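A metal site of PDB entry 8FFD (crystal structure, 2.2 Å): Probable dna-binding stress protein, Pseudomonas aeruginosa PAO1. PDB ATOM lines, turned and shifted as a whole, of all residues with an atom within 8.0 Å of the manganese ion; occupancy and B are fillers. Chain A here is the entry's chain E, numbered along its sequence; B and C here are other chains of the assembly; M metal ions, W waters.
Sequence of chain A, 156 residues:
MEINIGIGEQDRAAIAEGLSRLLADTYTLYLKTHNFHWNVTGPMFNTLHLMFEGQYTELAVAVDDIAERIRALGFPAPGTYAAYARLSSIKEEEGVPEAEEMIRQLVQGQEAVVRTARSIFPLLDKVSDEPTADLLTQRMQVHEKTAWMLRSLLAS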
ATOM      1  N   ALA A  60     -28.799   8.087   9.719  1.00  0.00           N
ATOM      2  CA  ALA A  60     -27.372   8.154  10.019  1.00  0.00           C
ATOM      3  C   ALA A  60     -27.009   7.158  11.102  1.00  0.00           C
ATOM      4  O   ALA A  60     -25.955   6.529  11.043  1.00  0.00           O
ATOM      5  CB  ALA A  60     -26.975   9.551  10.440  1.00  0.00           C
ATOM      6  N   VAL A  61     -27.877   6.984  12.088  1.00  0.00           N
ATOM      7  CA  VAL A  61     -27.598   5.995  13.141  1.00  0.00           C
ATOM      8  C   VAL A  61     -27.732   4.579  12.587  1.00  0.00           C
ATOM      9  O   VAL A  61     -26.937   3.698  12.894  1.00  0.00           O
ATOM     10  CB  VAL A  61     -28.508   6.226  14.369  1.00  0.00           C
ATOM     11  CG1 VAL A  61     -28.285   5.141  15.433  1.00  0.00           C
ATOM     12  CG2 VAL A  61     -28.293   7.639  15.000  1.00  0.00           C
ATOM     13  N   VAL A  63     -27.147   3.482   9.559  1.00  0.00           N
ATOM     14  CA  VAL A  63     -25.978   3.138   8.756  1.00  0.00           C
ATOM     15  C   VAL A  63     -24.856   2.639   9.659  1.00  0.00           C
ATOM     16  O   VAL A  63     -24.176   1.646   9.367  1.00  0.00           O
ATOM     17  CB  VAL A  63     -25.557   4.366   7.926  1.00  0.00           C
ATOM     18  CG1 VAL A  63     -24.134   4.276   7.471  1.00  0.00           C
ATOM     19  CG2 VAL A  63     -26.488   4.531   6.718  1.00  0.00           C
ATOM     20  N   ASP A  64     -24.651   3.344  10.775  1.00  0.00           N
ATOM     21  CA  ASP A  64     -23.605   2.955  11.718  1.00  0.00           C
ATOM     22  C   ASP A  64     -23.943   1.609  12.381  1.00  0.00           C
ATOM     23  O   ASP A  64     -23.059   0.785  12.590  1.00  0.00           O
ATOM     24  CB  ASP A  64     -23.393   4.074  12.761  1.00  0.00           C
ATOM     25  CG  ASP A  64     -22.140   3.854  13.630  1.00  0.00           C
ATOM     26  OD1 ASP A  64     -21.020   4.208  13.226  1.00  0.00           O
ATOM     27  OD2 ASP A  64     -22.263   3.326  14.748  1.00  0.00           O
ATOM     28  N   ASP A  65     -25.217   1.356  12.671  1.00  0.00           N
ATOM     29  CA  ASP A  65     -25.584   0.084  13.301  1.00  0.00           C
ATOM     30  C   ASP A  65     -25.420  -1.090  12.326  1.00  0.00           C
ATOM     31  O   ASP A  65     -24.989  -2.175  12.725  1.00  0.00           O
ATOM     32  CB  ASP A  65     -27.014   0.134  13.805  1.00  0.00           C
ATOM     33  CG  ASP A  65     -27.165   0.956  15.085  1.00  0.00           C
ATOM     34  OD1 ASP A  65     -26.173   1.221  15.796  1.00  0.00           O
ATOM     35  OD2 ASP A  65     -28.321   1.330  15.368  1.00  0.00           O
ATOM     36  N   ALA A  67     -23.424  -1.255   9.691  1.00  0.00           N
ATOM     37  CA  ALA A  67     -22.009  -1.418   9.370  1.00  0.00           C
ATOM     38  C   ALA A  67     -21.253  -2.119  10.487  1.00  0.00           C
ATOM     39  O   ALA A  67     -20.297  -2.847  10.215  1.00  0.00           O
ATOM     40  CB  ALA A  67     -21.375  -0.051   9.115  1.00  0.00           C
ATOM     41  N   GLU A  68     -21.626  -1.854  11.734  1.00  0.00           N
ATOM     42  CA  GLU A  68     -20.926  -2.496  12.837  1.00  0.00           C
ATOM     43  C   GLU A  68     -21.408  -3.903  13.087  1.00  0.00           C
ATOM     44  O   GLU A  68     -20.692  -4.678  13.724  1.00  0.00           O
ATOM     45  CB  GLU A  68     -21.053  -1.644  14.098  1.00  0.00           C
ATOM     46  CG  GLU A  68     -20.044  -0.490  14.029  1.00  0.00           C
ATOM     47  CD  GLU A  68     -20.255   0.581  15.069  1.00  0.00           C
ATOM     48  OE1 GLU A  68     -21.185   0.439  15.917  1.00  0.00           O
ATOM     49  OE2 GLU A  68     -19.497   1.579  15.030  1.00  0.00           O
ATOM     50  N   HIS B  34     -16.209   8.193   8.220  1.00  0.00           N
ATOM     51  CA  HIS B  34     -17.169   7.193   8.647  1.00  0.00           C
ATOM     52  C   HIS B  34     -16.641   5.800   8.356  1.00  0.00           C
ATOM     53  O   HIS B  34     -16.795   4.879   9.173  1.00  0.00           O
ATOM     54  CB  HIS B  34     -18.505   7.415   7.915  1.00  0.00           C
ATOM     55  CG  HIS B  34     -19.702   7.244   8.794  1.00  0.00           C
ATOM     56  ND1 HIS B  34     -20.956   7.658   8.419  1.00  0.00           N
ATOM     57  CD2 HIS B  34     -19.822   6.705  10.033  1.00  0.00           C
ATOM     58  CE1 HIS B  34     -21.813   7.385   9.388  1.00  0.00           C
ATOM     59  NE2 HIS B  34     -21.152   6.810  10.381  1.00  0.00           N
ATOM     60  N   HIS B  37     -13.733   4.924  10.548  1.00  0.00           N
ATOM     61  CA  HIS B  37     -14.251   4.685  11.889  1.00  0.00           C
ATOM     62  C   HIS B  37     -14.732   3.252  12.038  1.00  0.00           C
ATOM     63  O   HIS B  37     -14.502   2.618  13.068  1.00  0.00           O
ATOM     64  CB  HIS B  37     -15.369   5.691  12.192  1.00  0.00           C
ATOM     65  CG  HIS B  37     -16.319   5.242  13.263  1.00  0.00           C
ATOM     66  ND1 HIS B  37     -16.036   5.380  14.607  1.00  0.00           N
ATOM     67  CD2 HIS B  37     -17.549   4.670  13.196  1.00  0.00           C
ATOM     68  CE1 HIS B  37     -17.060   4.902  15.315  1.00  0.00           C
ATOM     69  NE2 HIS B  37     -17.983   4.478  14.478  1.00  0.00           N
ATOM     70  N   TRP B  38     -15.430   2.711  11.031  1.00  0.00           N
ATOM     71  CA  TRP B  38     -15.947   1.358  11.152  1.00  0.00           C
ATOM     72  C   TRP B  38     -14.847   0.317  11.061  1.00  0.00           C
ATOM     73  O   TRP B  38     -14.959  -0.754  11.675  1.00  0.00           O
ATOM     74  CB  TRP B  38     -16.949   1.046  10.042  1.00  0.00           C
ATOM     75  CG  TRP B  38     -18.183   1.818  10.081  1.00  0.00           C
ATOM     76  CD1 TRP B  38     -18.902   2.200  11.180  1.00  0.00           C
ATOM     77  CD2 TRP B  38     -18.882   2.322   8.952  1.00  0.00           C
ATOM     78  NE1 TRP B  38     -19.998   2.922  10.793  1.00  0.00           N
ATOM     79  CE2 TRP B  38     -20.001   3.021   9.427  1.00  0.00           C
ATOM     80  CE3 TRP B  38     -18.657   2.256   7.575  1.00  0.00           C
ATOM     81  CZ2 TRP B  38     -20.917   3.625   8.585  1.00  0.00           C
ATOM     82  CZ3 TRP B  38     -19.552   2.880   6.736  1.00  0.00           C
ATOM     83  CH2 TRP B  38     -20.672   3.534   7.238  1.00  0.00           C
ATOM     84  N   HIS B  49     -11.093   4.682  16.763  1.00  0.00           N
ATOM     85  CA  HIS B  49     -12.524   4.478  16.594  1.00  0.00           C
ATOM     86  C   HIS B  49     -13.302   5.654  17.173  1.00  0.00           C
ATOM     87  O   HIS B  49     -14.274   6.116  16.567  1.00  0.00           O
ATOM     88  CB  HIS B  49     -12.923   3.173  17.253  1.00  0.00           C
ATOM     89  CG  HIS B  49     -14.369   2.817  17.126  1.00  0.00           C
ATOM     90  ND1 HIS B  49     -14.948   2.446  15.943  1.00  0.00           N
ATOM     91  CD2 HIS B  49     -15.338   2.719  18.066  1.00  0.00           C
ATOM     92  CE1 HIS B  49     -16.213   2.148  16.144  1.00  0.00           C
ATOM     93  NE2 HIS B  49     -16.483   2.315  17.425  1.00  0.00           N
ATOM     94  N   LEU B  50     -12.892   6.155  18.342  1.00  0.00           N
ATOM     95  CA  LEU B  50     -13.581   7.266  18.960  1.00  0.00           C
ATOM     96  C   LEU B  50     -13.199   8.587  18.300  1.00  0.00           C
ATOM     97  O   LEU B  50     -14.059   9.441  18.072  1.00  0.00           O
ATOM     98  CB  LEU B  50     -13.295   7.326  20.456  1.00  0.00           C
ATOM     99  CG  LEU B  50     -13.750   6.111  21.290  1.00  0.00           C
ATOM    100  CD1 LEU B  50     -13.317   6.293  22.743  1.00  0.00           C
ATOM    101  CD2 LEU B  50     -15.265   5.866  21.209  1.00  0.00           C
ATOM    102  N   GLU B  53     -15.102   8.852  15.162  1.00  0.00           N
ATOM    103  CA  GLU B  53     -16.498   9.116  15.497  1.00  0.00           C
ATOM    104  C   GLU B  53     -16.728  10.600  15.694  1.00  0.00           C
ATOM    105  O   GLU B  53     -17.650  11.206  15.131  1.00  0.00           O
ATOM    106  CB  GLU B  53     -16.923   8.348  16.739  1.00  0.00           C
ATOM    107  CG  GLU B  53     -18.376   8.563  17.163  1.00  0.00           C
ATOM    108  CD  GLU B  53     -18.744   7.718  18.348  1.00  0.00           C
ATOM    109  OE1 GLU B  53     -18.300   8.032  19.468  1.00  0.00           O
ATOM    110  OE2 GLU B  53     -19.423   6.676  18.160  1.00  0.00           O
ATOM    111  N   TYR B  56     -16.521  12.438  12.178  1.00  0.00           N
ATOM    112  CA  TYR B  56     -17.614  12.301  11.227  1.00  0.00           C
ATOM    113  C   TYR B  56     -18.884  12.906  11.787  1.00  0.00           C
ATOM    114  O   TYR B  56     -19.708  13.407  11.023  1.00  0.00           O
ATOM    115  CB  TYR B  56     -17.846  10.839  10.823  1.00  0.00           C
ATOM    116  CG  TYR B  56     -18.664   9.962  11.742  1.00  0.00           C
ATOM    117  CD1 TYR B  56     -20.023  10.195  11.967  1.00  0.00           C
ATOM    118  CD2 TYR B  56     -18.098   8.833  12.319  1.00  0.00           C
ATOM    119  CE1 TYR B  56     -20.756   9.381  12.776  1.00  0.00           C
ATOM    120  CE2 TYR B  56     -18.835   8.005  13.121  1.00  0.00           C
ATOM    121  CZ  TYR B  56     -20.168   8.281  13.352  1.00  0.00           C
ATOM    122  OH  TYR B  56     -20.921   7.448  14.157  1.00  0.00           O
ATOM    123  N   LYS C 145     -20.709  -7.983  19.347  1.00  0.00           N
ATOM    124  CA  LYS C 145     -20.134  -6.668  19.095  1.00  0.00           C
ATOM    125  C   LYS C 145     -18.891  -6.443  19.932  1.00  0.00           C
ATOM    126  O   LYS C 145     -17.860  -5.985  19.433  1.00  0.00           O
ATOM    127  CB  LYS C 145     -21.148  -5.559  19.361  1.00  0.00           C
ATOM    128  CG  LYS C 145     -20.577  -4.180  19.113  1.00  0.00           C
ATOM    129  CD  LYS C 145     -21.641  -3.124  19.267  1.00  0.00           C
ATOM    130  CE  LYS C 145     -21.097  -1.714  18.994  1.00  0.00           C
ATOM    131  NZ  LYS C 145     -22.172  -0.674  18.879  1.00  0.00           N
ATOM    132  N   TRP C 148     -15.789  -8.220  18.676  1.00  0.00           N
ATOM    133  CA  TRP C 148     -15.162  -7.513  17.560  1.00  0.00           C
ATOM    134  C   TRP C 148     -14.277  -6.382  18.041  1.00  0.00           C
ATOM    135  O   TRP C 148     -13.145  -6.198  17.564  1.00  0.00           O
ATOM    136  CB  TRP C 148     -16.254  -6.967  16.610  1.00  0.00           C
ATOM    137  CG  TRP C 148     -15.840  -5.689  15.957  1.00  0.00           C
ATOM    138  CD1 TRP C 148     -14.756  -5.507  15.155  1.00  0.00           C
ATOM    139  CD2 TRP C 148     -16.490  -4.402  16.049  1.00  0.00           C
ATOM    140  NE1 TRP C 148     -14.670  -4.194  14.762  1.00  0.00           N
ATOM    141  CE2 TRP C 148     -15.735  -3.496  15.283  1.00  0.00           C
ATOM    142  CE3 TRP C 148     -17.631  -3.949  16.687  1.00  0.00           C
ATOM    143  CZ2 TRP C 148     -16.080  -2.149  15.159  1.00  0.00           C
ATOM    144  CZ3 TRP C 148     -17.983  -2.603  16.556  1.00  0.00           C
ATOM    145  CH2 TRP C 148     -17.198  -1.719  15.809  1.00  0.00           C
HETATM  146 MN    MN M   1     -20.089   3.703  15.307  1.00  0.00          MN
HETATM  147  O   HOH W   1     -20.795   5.637  16.166  1.00  0.00           O
HETATM  148  O   HOH W   2     -19.582   3.307  17.720  1.00  0.00           O
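NZ of Lys 145 of chain C is in salt-bridge range of OE1 of Glu 68 (3.3 Å). OD1 of Asp 64 sits close to OH of Tyr 56 of chain B (3.4 Å). NE1 of Trp 38 of chain B lies close to OD1 of Asp 64 (2.9 Å). The backbone carbonyl oxygen of His 49 of chain B is in hydrogen-bond range of a ring nitrogen (ND1) of His 37 of chain B (2.7 Å).
Three residues have an atom within 4 Å of the manganese ion: Asp 64, Glu 68 and His 37 of chain B. The nearest printed residue that does not touch the manganese ion is Tyr 56 of chain B (4.005 Å).
The manganese ion is bound by OE2 of Glu 68. The manganese ion is bound by water W1 (2.2 Å). The manganese ion is bound by the side-chain carboxylate (OD2) of Asp 64 (2.3 Å). The side-chain carboxylate (OD1) of Asp 64 binds the manganese ion, 2.3 Å away. A ring nitrogen (NE2) of His 37 of chain B is bound to the manganese ion (2.4 Å). The manganese ion is bound by water W2, 2.5 Å away.
Water W2 bridges a ring nitrogen (NE2) of His 49 of chain B and the side-chain carboxylate (OE2) of Glu 53 of chain B. Water W1 bridges the side-chain carboxylate (OE2) of Glu 53 of chain B and the side-chain hydroxyl (OH) of Tyr 56 of chain B.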
